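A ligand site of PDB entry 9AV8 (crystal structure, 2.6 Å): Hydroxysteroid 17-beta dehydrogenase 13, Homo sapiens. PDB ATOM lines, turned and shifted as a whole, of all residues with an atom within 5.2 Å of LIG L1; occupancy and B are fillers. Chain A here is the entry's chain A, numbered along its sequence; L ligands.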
ATOM      1  N   GLY A  44       6.468  -0.593  15.251  1.00  0.00           N
ATOM      2  CA  GLY A  44       6.096  -0.832  13.860  1.00  0.00           C
ATOM      3  C   GLY A  44       6.389   0.390  13.017  1.00  0.00           C
ATOM      4  O   GLY A  44       5.598   0.766  12.148  1.00  0.00           O
ATOM      5  N   ALA A  45       7.544   1.024  13.281  1.00  0.00           N
ATOM      6  CA  ALA A  45       7.959   2.240  12.587  1.00  0.00           C
ATOM      7  C   ALA A  45       8.983   2.032  11.481  1.00  0.00           C
ATOM      8  O   ALA A  45       9.691   2.976  11.119  1.00  0.00           O
ATOM      9  CB  ALA A  45       8.475   3.273  13.586  1.00  0.00           C
ATOM     10  N   GLY A  46       9.048   0.821  10.941  1.00  0.00           N
ATOM     11  CA  GLY A  46       9.960   0.534   9.842  1.00  0.00           C
ATOM     12  C   GLY A  46       9.372   0.818   8.469  1.00  0.00           C
ATOM     13  O   GLY A  46      10.114   0.870   7.486  1.00  0.00           O
ATOM     14  N   HIS A  47       8.042   0.995   8.391  1.00  0.00           N
ATOM     15  CA  HIS A  47       7.359   1.249   7.137  1.00  0.00           C
ATOM     16  C   HIS A  47       5.917   1.698   7.370  1.00  0.00           C
ATOM     17  O   HIS A  47       5.353   1.487   8.456  1.00  0.00           O
ATOM     18  CB  HIS A  47       7.400  -0.037   6.286  1.00  0.00           C
ATOM     19  CG  HIS A  47       6.761   0.063   4.933  1.00  0.00           C
ATOM     20  ND1 HIS A  47       6.931   1.187   4.137  1.00  0.00           N
ATOM     21  CD2 HIS A  47       6.030  -0.845   4.259  1.00  0.00           C
ATOM     22  CE1 HIS A  47       6.262   0.941   3.026  1.00  0.00           C
ATOM     23  NE2 HIS A  47       5.710  -0.280   3.045  1.00  0.00           N
ATOM     24  N   GLY A  48       5.351   2.341   6.348  1.00  0.00           N
ATOM     25  CA  GLY A  48       3.972   2.778   6.283  1.00  0.00           C
ATOM     26  C   GLY A  48       3.537   3.831   7.284  1.00  0.00           C
ATOM     27  O   GLY A  48       4.179   4.876   7.399  1.00  0.00           O
ATOM     28  N   ILE A  49       2.428   3.547   8.005  1.00  0.00           N
ATOM     29  CA  ILE A  49       1.867   4.446   9.005  1.00  0.00           C
ATOM     30  C   ILE A  49       2.858   4.711  10.149  1.00  0.00           C
ATOM     31  O   ILE A  49       2.882   5.811  10.672  1.00  0.00           O
ATOM     32  CB  ILE A  49       0.462   4.002   9.516  1.00  0.00           C
ATOM     33  CG1 ILE A  49      -0.441   3.567   8.345  1.00  0.00           C
ATOM     34  CG2 ILE A  49      -0.194   5.111  10.366  1.00  0.00           C
ATOM     35  CD1 ILE A  49      -1.732   3.014   8.749  1.00  0.00           C
ATOM     36  N   GLY A  50       3.686   3.731  10.485  1.00  0.00           N
ATOM     37  CA  GLY A  50       4.680   3.902  11.539  1.00  0.00           C
ATOM     38  C   GLY A  50       5.867   4.739  11.106  1.00  0.00           C
ATOM     39  O   GLY A  50       6.363   5.554  11.879  1.00  0.00           O
ATOM     40  N   TRP A  67      10.828   1.091  17.371  1.00  0.00           N
ATOM     41  CA  TRP A  67      10.824  -0.358  17.589  1.00  0.00           C
ATOM     42  C   TRP A  67      10.253  -1.088  16.381  1.00  0.00           C
ATOM     43  O   TRP A  67       9.265  -0.625  15.802  1.00  0.00           O
ATOM     44  CB  TRP A  67      10.006  -0.696  18.833  1.00  0.00           C
ATOM     45  CG  TRP A  67      10.692  -0.457  20.148  1.00  0.00           C
ATOM     46  CD1 TRP A  67      11.791   0.318  20.390  1.00  0.00           C
ATOM     47  CD2 TRP A  67      10.292  -0.979  21.414  1.00  0.00           C
ATOM     48  NE1 TRP A  67      12.122   0.282  21.728  1.00  0.00           N
ATOM     49  CE2 TRP A  67      11.216  -0.512  22.377  1.00  0.00           C
ATOM     50  CE3 TRP A  67       9.256  -1.812  21.840  1.00  0.00           C
ATOM     51  CZ2 TRP A  67      11.130  -0.855  23.725  1.00  0.00           C
ATOM     52  CZ3 TRP A  67       9.168  -2.149  23.176  1.00  0.00           C
ATOM     53  CH2 TRP A  67      10.104  -1.676  24.100  1.00  0.00           C
ATOM     54  N   ASP A  68      10.866  -2.210  15.978  1.00  0.00           N
ATOM     55  CA  ASP A  68      10.413  -2.997  14.826  1.00  0.00           C
ATOM     56  C   ASP A  68      11.158  -4.354  14.720  1.00  0.00           C
ATOM     57  O   ASP A  68      12.204  -4.539  15.350  1.00  0.00           O
ATOM     58  CB  ASP A  68      10.627  -2.187  13.531  1.00  0.00           C
ATOM     59  CG  ASP A  68       9.701  -2.585  12.404  1.00  0.00           C
ATOM     60  OD1 ASP A  68       8.731  -1.847  12.140  1.00  0.00           O
ATOM     61  OD2 ASP A  68       9.945  -3.630  11.767  1.00  0.00           O
ATOM     62  N   ILE A  69      10.636  -5.295  13.934  1.00  0.00           N
ATOM     63  CA  ILE A  69      11.315  -6.573  13.686  1.00  0.00           C
ATOM     64  C   ILE A  69      12.272  -6.471  12.479  1.00  0.00           C
ATOM     65  O   ILE A  69      13.247  -7.228  12.389  1.00  0.00           O
ATOM     66  CB  ILE A  69      10.310  -7.743  13.527  1.00  0.00           C
ATOM     67  CG1 ILE A  69       9.247  -7.423  12.459  1.00  0.00           C
ATOM     68  CG2 ILE A  69       9.687  -8.111  14.859  1.00  0.00           C
ATOM     69  CD1 ILE A  69       9.392  -8.239  11.119  1.00  0.00           C
ATOM     70  N   ASN A  70      12.004  -5.520  11.553  1.00  0.00           N
ATOM     71  CA  ASN A  70      12.769  -5.235  10.348  1.00  0.00           C
ATOM     72  C   ASN A  70      13.884  -4.303  10.712  1.00  0.00           C
ATOM     73  O   ASN A  70      13.653  -3.102  10.790  1.00  0.00           O
ATOM     74  CB  ASN A  70      11.869  -4.560   9.310  1.00  0.00           C
ATOM     75  CG  ASN A  70      12.441  -4.526   7.932  1.00  0.00           C
ATOM     76  OD1 ASN A  70      13.631  -4.297   7.729  1.00  0.00           O
ATOM     77  ND2 ASN A  70      11.593  -4.736   6.938  1.00  0.00           N
ATOM     78  N   VAL A  93      12.825  -4.941  18.238  1.00  0.00           N
ATOM     79  CA  VAL A  93      11.990  -5.552  19.270  1.00  0.00           C
ATOM     80  C   VAL A  93      10.808  -6.292  18.682  1.00  0.00           C
ATOM     81  O   VAL A  93      10.059  -5.715  17.903  1.00  0.00           O
ATOM     82  CB  VAL A  93      11.483  -4.480  20.275  1.00  0.00           C
ATOM     83  CG1 VAL A  93      10.762  -5.127  21.452  1.00  0.00           C
ATOM     84  CG2 VAL A  93      12.597  -3.573  20.752  1.00  0.00           C
ATOM     85  N   ASP A  94      10.617  -7.550  19.078  1.00  0.00           N
ATOM     86  CA  ASP A  94       9.445  -8.324  18.645  1.00  0.00           C
ATOM     87  C   ASP A  94       8.311  -7.789  19.499  1.00  0.00           C
ATOM     88  O   ASP A  94       8.142  -8.206  20.641  1.00  0.00           O
ATOM     89  CB  ASP A  94       9.659  -9.815  18.942  1.00  0.00           C
ATOM     90  CG  ASP A  94       8.565 -10.742  18.452  1.00  0.00           C
ATOM     91  OD1 ASP A  94       7.691 -10.274  17.685  1.00  0.00           O
ATOM     92  OD2 ASP A  94       8.597 -11.943  18.813  1.00  0.00           O
ATOM     93  N   CYS A  95       7.551  -6.818  18.960  1.00  0.00           N
ATOM     94  CA  CYS A  95       6.482  -6.129  19.676  1.00  0.00           C
ATOM     95  C   CYS A  95       5.223  -6.972  19.931  1.00  0.00           C
ATOM     96  O   CYS A  95       4.148  -6.434  20.198  1.00  0.00           O
ATOM     97  CB  CYS A  95       6.141  -4.799  19.000  1.00  0.00           C
ATOM     98  SG  CYS A  95       7.562  -3.704  18.752  1.00  0.00           S
ATOM     99  N   GLY A  96       5.379  -8.288  19.893  1.00  0.00           N
ATOM    100  CA  GLY A  96       4.336  -9.253  20.215  1.00  0.00           C
ATOM    101  C   GLY A  96       4.737 -10.118  21.400  1.00  0.00           C
ATOM    102  O   GLY A  96       3.867 -10.627  22.122  1.00  0.00           O
ATOM    103  N   ASN A 121       1.645   1.365  16.991  1.00  0.00           N
ATOM    104  CA  ASN A 121       1.327   1.245  15.582  1.00  0.00           C
ATOM    105  C   ASN A 121       1.327  -0.199  15.090  1.00  0.00           C
ATOM    106  O   ASN A 121       0.313  -0.645  14.557  1.00  0.00           O
ATOM    107  CB  ASN A 121       2.260   2.133  14.751  1.00  0.00           C
ATOM    108  CG  ASN A 121       2.019   2.125  13.269  1.00  0.00           C
ATOM    109  OD1 ASN A 121       1.215   2.905  12.754  1.00  0.00           O
ATOM    110  ND2 ASN A 121       2.747   1.288  12.535  1.00  0.00           N
ATOM    111  N   ALA A 122       2.443  -0.948  15.332  1.00  0.00           N
ATOM    112  CA  ALA A 122       2.650  -2.350  14.911  1.00  0.00           C
ATOM    113  C   ALA A 122       1.381  -3.183  14.758  1.00  0.00           C
ATOM    114  O   ALA A 122       0.449  -3.049  15.549  1.00  0.00           O
ATOM    115  CB  ALA A 122       3.615  -3.061  15.861  1.00  0.00           C
ATOM    116  N   GLY A 123       1.346  -3.997  13.706  1.00  0.00           N
ATOM    117  CA  GLY A 123       0.228  -4.860  13.397  1.00  0.00           C
ATOM    118  C   GLY A 123       0.584  -5.937  12.399  1.00  0.00           C
ATOM    119  O   GLY A 123       1.594  -5.839  11.682  1.00  0.00           O
ATOM    120  N   THR A 124      -0.236  -7.001  12.343  1.00  0.00           N
ATOM    121  CA  THR A 124      -0.069  -8.114  11.399  1.00  0.00           C
ATOM    122  C   THR A 124      -1.457  -8.552  10.885  1.00  0.00           C
ATOM    123  O   THR A 124      -2.455  -8.463  11.605  1.00  0.00           O
ATOM    124  CB  THR A 124       0.811  -9.242  11.998  1.00  0.00           C
ATOM    125  OG1 THR A 124       1.477  -9.945  10.951  1.00  0.00           O
ATOM    126  CG2 THR A 124       0.037 -10.213  12.852  1.00  0.00           C
ATOM    127  N   ILE A 144       0.223  -9.391  18.553  1.00  0.00           N
ATOM    128  CA  ILE A 144       0.778  -8.127  18.076  1.00  0.00           C
ATOM    129  C   ILE A 144      -0.209  -6.956  18.163  1.00  0.00           C
ATOM    130  O   ILE A 144       0.135  -5.866  18.661  1.00  0.00           O
ATOM    131  CB  ILE A 144       1.303  -8.344  16.618  1.00  0.00           C
ATOM    132  CG1 ILE A 144       2.514  -9.276  16.608  1.00  0.00           C
ATOM    133  CG2 ILE A 144       1.628  -7.018  15.917  1.00  0.00           C
ATOM    134  CD1 ILE A 144       2.830  -9.810  15.279  1.00  0.00           C
ATOM    135  N   ASN A 145      -1.438  -7.184  17.677  1.00  0.00           N
ATOM    136  CA  ASN A 145      -2.493  -6.182  17.591  1.00  0.00           C
ATOM    137  C   ASN A 145      -3.096  -5.737  18.920  1.00  0.00           C
ATOM    138  O   ASN A 145      -3.618  -4.614  18.973  1.00  0.00           O
ATOM    139  CB  ASN A 145      -3.601  -6.643  16.661  1.00  0.00           C
ATOM    140  CG  ASN A 145      -3.186  -6.878  15.245  1.00  0.00           C
ATOM    141  OD1 ASN A 145      -2.071  -6.557  14.837  1.00  0.00           O
ATOM    142  ND2 ASN A 145      -4.069  -7.468  14.456  1.00  0.00           N
ATOM    143  N   VAL A 171      -3.122   2.577  17.671  1.00  0.00           N
ATOM    144  CA  VAL A 171      -3.423   2.538  16.248  1.00  0.00           C
ATOM    145  C   VAL A 171      -4.268   1.313  15.882  1.00  0.00           C
ATOM    146  O   VAL A 171      -3.783   0.177  15.900  1.00  0.00           O
ATOM    147  CB  VAL A 171      -2.164   2.648  15.362  1.00  0.00           C
ATOM    148  CG1 VAL A 171      -2.542   2.614  13.884  1.00  0.00           C
ATOM    149  CG2 VAL A 171      -1.380   3.911  15.692  1.00  0.00           C
ATOM    150  N   ALA A 172      -5.538   1.555  15.572  1.00  0.00           N
ATOM    151  CA  ALA A 172      -6.507   0.512  15.190  1.00  0.00           C
ATOM    152  C   ALA A 172      -7.062   0.837  13.744  1.00  0.00           C
ATOM    153  O   ALA A 172      -6.467   1.673  13.078  1.00  0.00           O
ATOM    154  CB  ALA A 172      -7.603   0.421  16.261  1.00  0.00           C
ATOM    155  N   SER A 173      -8.129   0.201  13.253  1.00  0.00           N
ATOM    156  CA  SER A 173      -8.689   0.487  11.931  1.00  0.00           C
ATOM    157  C   SER A 173     -10.216   0.634  12.052  1.00  0.00           C
ATOM    158  O   SER A 173     -10.760   0.447  13.138  1.00  0.00           O
ATOM    159  CB  SER A 173      -8.346  -0.674  10.984  1.00  0.00           C
ATOM    160  OG  SER A 173      -9.085  -0.731   9.774  1.00  0.00           O
ATOM    161  N   TYR A 186      -8.424 -10.534  12.339  1.00  0.00           N
ATOM    162  CA  TYR A 186      -7.874  -9.183  12.340  1.00  0.00           C
ATOM    163  C   TYR A 186      -8.869  -8.175  12.920  1.00  0.00           C
ATOM    164  O   TYR A 186      -8.480  -7.337  13.713  1.00  0.00           O
ATOM    165  CB  TYR A 186      -7.449  -8.800  10.931  1.00  0.00           C
ATOM    166  CG  TYR A 186      -7.047  -7.348  10.766  1.00  0.00           C
ATOM    167  CD1 TYR A 186      -5.782  -6.921  11.107  1.00  0.00           C
ATOM    168  CD2 TYR A 186      -7.931  -6.423  10.226  1.00  0.00           C
ATOM    169  CE1 TYR A 186      -5.390  -5.603  10.916  1.00  0.00           C
ATOM    170  CE2 TYR A 186      -7.560  -5.098  10.057  1.00  0.00           C
ATOM    171  CZ  TYR A 186      -6.289  -4.685  10.391  1.00  0.00           C
ATOM    172  OH  TYR A 186      -5.924  -3.385  10.196  1.00  0.00           O
ATOM    173  N   LYS A 190      -8.542  -5.759  16.168  1.00  0.00           N
ATOM    174  CA  LYS A 190      -8.692  -4.323  16.024  1.00  0.00           C
ATOM    175  C   LYS A 190      -9.826  -3.799  16.912  1.00  0.00           C
ATOM    176  O   LYS A 190      -9.672  -2.747  17.510  1.00  0.00           O
ATOM    177  CB  LYS A 190      -8.850  -3.910  14.559  1.00  0.00           C
ATOM    178  CG  LYS A 190      -7.568  -4.048  13.747  1.00  0.00           C
ATOM    179  CD  LYS A 190      -6.498  -3.065  14.188  1.00  0.00           C
ATOM    180  CE  LYS A 190      -5.193  -3.730  14.594  1.00  0.00           C
ATOM    181  NZ  LYS A 190      -4.269  -2.773  15.273  1.00  0.00           N
ATOM    182  N   PRO A 219      -8.227   4.538  10.594  1.00  0.00           N
ATOM    183  CA  PRO A 219      -8.391   4.854   9.174  1.00  0.00           C
ATOM    184  C   PRO A 219      -9.022   3.723   8.353  1.00  0.00           C
ATOM    185  O   PRO A 219      -9.232   2.633   8.874  1.00  0.00           O
ATOM    186  CB  PRO A 219      -6.963   5.165   8.725  1.00  0.00           C
ATOM    187  CG  PRO A 219      -6.064   4.456   9.718  1.00  0.00           C
ATOM    188  CD  PRO A 219      -6.906   3.948  10.859  1.00  0.00           C
ATOM    189  N   VAL A 220      -9.347   3.995   7.072  1.00  0.00           N
ATOM    190  CA  VAL A 220      -9.898   2.980   6.157  1.00  0.00           C
ATOM    191  C   VAL A 220      -8.702   2.304   5.386  1.00  0.00           C
ATOM    192  O   VAL A 220      -7.681   2.103   6.037  1.00  0.00           O
ATOM    193  CB  VAL A 220     -11.058   3.550   5.294  1.00  0.00           C
ATOM    194  CG1 VAL A 220     -12.237   3.937   6.160  1.00  0.00           C
ATOM    195  CG2 VAL A 220     -10.597   4.738   4.454  1.00  0.00           C
ATOM    196  N   PHE A 221      -8.788   1.945   4.068  1.00  0.00           N
ATOM    197  CA  PHE A 221      -7.641   1.337   3.406  1.00  0.00           C
ATOM    198  C   PHE A 221      -6.537   2.343   3.210  1.00  0.00           C
ATOM    199  O   PHE A 221      -6.763   3.397   2.627  1.00  0.00           O
ATOM    200  CB  PHE A 221      -7.978   0.677   2.065  1.00  0.00           C
ATOM    201  CG  PHE A 221      -6.888  -0.289   1.653  1.00  0.00           C
ATOM    202  CD1 PHE A 221      -5.903   0.092   0.768  1.00  0.00           C
ATOM    203  CD2 PHE A 221      -6.802  -1.548   2.230  1.00  0.00           C
ATOM    204  CE1 PHE A 221      -4.876  -0.783   0.423  1.00  0.00           C
ATOM    205  CE2 PHE A 221      -5.782  -2.425   1.869  1.00  0.00           C
ATOM    206  CZ  PHE A 221      -4.827  -2.035   0.977  1.00  0.00           C
ATOM    207  N   VAL A 222      -5.345   2.012   3.672  1.00  0.00           N
ATOM    208  CA  VAL A 222      -4.179   2.847   3.468  1.00  0.00           C
ATOM    209  C   VAL A 222      -3.270   2.099   2.502  1.00  0.00           C
ATOM    210  O   VAL A 222      -3.017   0.895   2.677  1.00  0.00           O
ATOM    211  CB  VAL A 222      -3.457   3.213   4.779  1.00  0.00           C
ATOM    212  CG1 VAL A 222      -2.374   4.232   4.514  1.00  0.00           C
ATOM    213  CG2 VAL A 222      -4.442   3.734   5.798  1.00  0.00           C
ATOM    214  N   THR A 224      -0.317   0.892   1.770  1.00  0.00           N
ATOM    215  CA  THR A 224       1.001   0.605   2.373  1.00  0.00           C
ATOM    216  C   THR A 224       1.569  -0.760   1.971  1.00  0.00           C
ATOM    217  O   THR A 224       2.760  -0.996   2.156  1.00  0.00           O
ATOM    218  CB  THR A 224       0.933   0.647   3.897  1.00  0.00           C
ATOM    219  OG1 THR A 224       0.028  -0.357   4.367  1.00  0.00           O
ATOM    220  CG2 THR A 224       0.556   2.016   4.441  1.00  0.00           C
ATOM    221  N   GLY A 225       0.724  -1.641   1.461  1.00  0.00           N
ATOM    222  CA  GLY A 225       1.146  -2.990   1.137  1.00  0.00           C
ATOM    223  C   GLY A 225       0.876  -3.975   2.254  1.00  0.00           C
ATOM    224  O   GLY A 225       1.262  -5.137   2.136  1.00  0.00           O
ATOM    225  N   PHE A 226       0.193  -3.529   3.331  1.00  0.00           N
ATOM    226  CA  PHE A 226      -0.232  -4.309   4.494  1.00  0.00           C
ATOM    227  C   PHE A 226      -1.089  -5.494   3.960  1.00  0.00           C
ATOM    228  O   PHE A 226      -0.813  -6.656   4.228  1.00  0.00           O
ATOM    229  CB  PHE A 226      -1.006  -3.384   5.454  1.00  0.00           C
ATOM    230  CG  PHE A 226      -1.383  -3.925   6.801  1.00  0.00           C
ATOM    231  CD1 PHE A 226      -0.421  -4.407   7.665  1.00  0.00           C
ATOM    232  CD2 PHE A 226      -2.688  -3.868   7.245  1.00  0.00           C
ATOM    233  CE1 PHE A 226      -0.770  -4.874   8.924  1.00  0.00           C
ATOM    234  CE2 PHE A 226      -3.030  -4.340   8.507  1.00  0.00           C
ATOM    235  CZ  PHE A 226      -2.076  -4.841   9.333  1.00  0.00           C
HETATM  236  P1  LIG L   1       2.982  -1.899   7.148  1.00  0.00           P
HETATM  237  O1  LIG L   1       3.329  -0.911   6.097  1.00  0.00           O
HETATM  238  O2  LIG L   1       2.882  -3.323   6.782  1.00  0.00           O
HETATM  239  O3  LIG L   1       4.043  -1.700   8.321  1.00  0.00           O
HETATM  240  C1  LIG L   1       3.779  -2.228   9.640  1.00  0.00           C
HETATM  241  C2  LIG L   1       5.089  -2.390  10.362  1.00  0.00           C
HETATM  242  O4  LIG L   1       4.884  -3.172  11.558  1.00  0.00           O
HETATM  243  C3  LIG L   1       6.207  -3.080   9.559  1.00  0.00           C
HETATM  244  O5  LIG L   1       7.321  -2.210   9.348  1.00  0.00           O
HETATM  245  C4  LIG L   1       6.554  -4.323  10.398  1.00  0.00           C
HETATM  246  O6  LIG L   1       7.946  -4.626  10.410  1.00  0.00           O
HETATM  247  C5  LIG L   1       6.053  -3.937  11.785  1.00  0.00           C
HETATM  248  N1  LIG L   1       5.722  -5.085  12.629  1.00  0.00           N
HETATM  249  C6  LIG L   1       4.902  -6.137  12.320  1.00  0.00           C
HETATM  250  N2  LIG L   1       4.886  -7.086  13.224  1.00  0.00           N
HETATM  251  C7  LIG L   1       5.753  -6.624  14.202  1.00  0.00           C
HETATM  252  C8  LIG L   1       6.194  -7.180  15.416  1.00  0.00           C
HETATM  253  N3  LIG L   1       5.845  -8.390  15.859  1.00  0.00           N
HETATM  254  N4  LIG L   1       7.078  -6.460  16.145  1.00  0.00           N
HETATM  255  C9  LIG L   1       7.482  -5.280  15.687  1.00  0.00           C
HETATM  256  N5  LIG L   1       7.139  -4.653  14.551  1.00  0.00           N
HETATM  257  C10 LIG L   1       6.267  -5.390  13.851  1.00  0.00           C
HETATM  258  O7  LIG L   1       1.625  -1.436   7.866  1.00  0.00           O
HETATM  259  P2  LIG L   1       0.845  -0.045   8.009  1.00  0.00           P
HETATM  260  O8  LIG L   1       1.746   0.972   8.594  1.00  0.00           O
HETATM  261  O9  LIG L   1       0.139   0.241   6.742  1.00  0.00           O
HETATM  262  O10 LIG L   1      -0.215  -0.404   9.150  1.00  0.00           O
HETATM  263  C11 LIG L   1       0.253  -0.953  10.402  1.00  0.00           C
HETATM  264  C12 LIG L   1      -0.754  -0.673  11.482  1.00  0.00           C
HETATM  265  O11 LIG L   1      -1.744   0.256  10.985  1.00  0.00           O
HETATM  266  C13 LIG L   1      -1.527  -1.898  11.996  1.00  0.00           C
HETATM  267  O12 LIG L   1      -1.722  -1.835  13.401  1.00  0.00           O
HETATM  268  C14 LIG L   1      -2.839  -1.823  11.205  1.00  0.00           C
HETATM  269  O13 LIG L   1      -3.920  -2.474  11.868  1.00  0.00           O
HETATM  270  C15 LIG L   1      -3.033  -0.305  11.080  1.00  0.00           C
HETATM  271  N6  LIG L   1      -3.833   0.073   9.862  1.00  0.00           N
HETATM  272  C16 LIG L   1      -3.339  -0.205   8.641  1.00  0.00           C
HETATM  273  C17 LIG L   1      -4.096   0.043   7.506  1.00  0.00           C
HETATM  274  C18 LIG L   1      -3.549  -0.227   6.131  1.00  0.00           C
HETATM  275  O14 LIG L   1      -4.318  -0.576   5.218  1.00  0.00           O
HETATM  276  N7  LIG L   1      -2.229  -0.078   5.957  1.00  0.00           N
HETATM  277  C19 LIG L   1      -5.369   0.581   7.672  1.00  0.00           C
HETATM  278  C20 LIG L   1      -5.843   0.879   8.939  1.00  0.00           C
HETATM  279  C21 LIG L   1      -5.060   0.616  10.031  1.00  0.00           C
HETATM  280  C1  LG2 L   2      -8.429  -3.372   5.075  1.00  0.00           C
HETATM  281  N1  LG2 L   2      -8.600  -4.934   3.510  1.00  0.00           N
HETATM  282  C2  LG2 L   2     -10.077  -1.146   5.528  1.00  0.00           C
HETATM  283  C3  LG2 L   2      -9.060  -1.447   6.409  1.00  0.00           C
HETATM  284  C4  LG2 L   2      -9.475  -3.084   4.178  1.00  0.00           C
HETATM  285  C5  LG2 L   2     -13.587  -0.748   5.257  1.00  0.00           C
HETATM  286  C6  LG2 L   2     -10.300  -1.956   4.415  1.00  0.00           C
HETATM  287  C7  LG2 L   2     -15.361   0.739   5.950  1.00  0.00           C
HETATM  288  C8  LG2 L   2     -14.075   1.229   3.969  1.00  0.00           C
HETATM  289  C9  LG2 L   2     -14.592  -0.414   6.141  1.00  0.00           C
HETATM  290  C10 LG2 L   2     -19.684   0.676   7.743  1.00  0.00           C
HETATM  291  C11 LG2 L   2      -8.500  -6.181   2.761  1.00  0.00           C
HETATM  292  C12 LG2 L   2      -7.870  -4.604   4.585  1.00  0.00           C
HETATM  293  C13 LG2 L   2      -8.230  -2.551   6.197  1.00  0.00           C
HETATM  294  N2  LG2 L   2      -9.579  -4.029   3.205  1.00  0.00           N
HETATM  295  N3  LG2 L   2     -11.414  -1.759   3.551  1.00  0.00           N
HETATM  296  S1  LG2 L   2     -12.063  -0.349   3.032  1.00  0.00           S
HETATM  297  O1  LG2 L   2     -11.049   0.663   3.096  1.00  0.00           O
HETATM  298  O2  LG2 L   2     -12.672  -0.644   1.773  1.00  0.00           O
HETATM  299  C14 LG2 L   2     -13.340   0.080   4.175  1.00  0.00           C
HETATM  300  C15 LG2 L   2     -15.091   1.554   4.859  1.00  0.00           C
HETATM  301 CL1  LG2 L   2     -14.895  -1.438   7.505  1.00  0.00          CL
HETATM  302  C16 LG2 L   2      -7.115  -2.743   7.188  1.00  0.00           C
HETATM  303  O3  LG2 L   2      -7.142  -2.165   8.255  1.00  0.00           O
HETATM  304  O4  LG2 L   2      -6.207  -3.616   6.879  1.00  0.00           O
HETATM  305  O5  LG2 L   2     -16.351   0.977   6.868  1.00  0.00           O
HETATM  306  C17 LG2 L   2     -17.215   2.114   6.646  1.00  0.00           C
HETATM  307  C18 LG2 L   2     -18.186   2.212   7.795  1.00  0.00           C
HETATM  308  C19 LG2 L   2     -18.440   0.936   8.616  1.00  0.00           C
HETATM  309  C20 LG2 L   2     -19.650   2.148   7.335  1.00  0.00           C
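NZ of Lys 190 is in hydrogen-bond range of O of Val 171 (3.1 Å). OD2 of Asp 68 lies within hydrogen-bond range of N of Asn 70 (2.8 Å). OG of Ser 173 is in hydrogen-bond range of O of Pro 219 (3.5 Å). The backbone carbonyl oxygen of Gly 44 is in hydrogen-bond range of the side-chain amide nitrogen of Asn 121 (2.9 Å). OG1 of Thr 224 lies within hydrogen-bond range of N of Phe 226, at 3.3 Å. The side-chain carboxylate (OD1) of Asp 68 lies within hydrogen-bond range of the backbone NH (N) of Gly 46 (2.9 Å). The side-chain carboxylate of Asp 68 sits at hydrogen-bond distance from the backbone NH of Ala 45 (3.3 Å). N of Gly 44 is in hydrogen-bond range of O of Trp 67 (2.9 Å).
An oxygen (O5) of LIG L1 sits at hydrogen-bond distance from the backbone NH (N) of His 47, 3.4 Å away. O9 of LIG L1 lies within hydrogen-bond range of OG1 of Thr 224, 2.5 Å away. OG of Ser 173 lies within hydrogen-bond range of O3 of LG2 L2 (2.9 Å). An oxygen (O3) of LG2 L2 lies within hydrogen-bond range of the side-chain hydroxyl (OH) of Tyr 186 (2.6 Å). N of Phe 221 lies within hydrogen-bond range of O1 of LG2 L2 (2.8 Å). N of Ile 49 is in hydrogen-bond range of O8 of LIG L1. The side-chain amino group (NZ) of Lys 190 lies within hydrogen-bond range of an oxygen (O12) of LIG L1, 3.3 Å away. The backbone carbonyl oxygen of Ala 122 is in hydrogen-bond range of an oxygen (O12) of LIG L1 (3.3 Å). O6 of LIG L1 sits at hydrogen-bond distance from OD2 of Asp 68 (2.6 Å). An oxygen (O14) of LIG L1 is in hydrogen-bond range of the backbone NH (N) of Val 222, at 3.2 Å. A nitrogen (N4) of LIG L1 sits at hydrogen-bond distance from the backbone NH (N) of Cys 95 (2.9 Å). An oxygen (O13) of LIG L1 lies within hydrogen-bond range of the side-chain hydroxyl of Tyr 186, at 2.8 Å. The backbone carbonyl oxygen (O) of Asn 121 is in hydrogen-bond range of an oxygen (O12) of LIG L1, 2.6 Å away. OD1 of Asp 94 lies within hydrogen-bond range of N3 of LIG L1, at 3.2 Å.
Gly 44 touches LIG L1 (CA to O4, 3.5 Å). Gly 46 touches LIG L1 (C to O5, 3.8 Å). Gly 48 touches LIG L1 (C to O8, 3.6 Å). N of Gly 50 touches O8 of LIG L1 (3.9 Å). CG2 of Ile 69 touches N4 of LIG L1 (3.3 Å). Val 93 touches LIG L1. Gly 123 touches LIG L1. Ile 144 touches LIG L1. Val 171 touches LIG L1. Ala 172 touches LIG L1. Ser 173 touches LIG L1. CG of Pro 219 touches C20 of LIG L1, 3.7 Å away. O of Val 220 touches C19 of LIG L1, 3.2 Å away. Phe 226 touches LIG L1. 25 residues have an atom within 4 Å of LIG L1: Gly 44, Gly 46, His 47, Gly 48, Ile 49, Gly 50, Asp 68, Ile 69, Val 93, Asp 94, Cys 95, Asn 121, Ala 122, Gly 123, Ile 144, Val 171, Ala 172, Ser 173, Tyr 186, Lys 190, Pro 219, Val 220, Val 222, Thr 224 and Phe 226.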
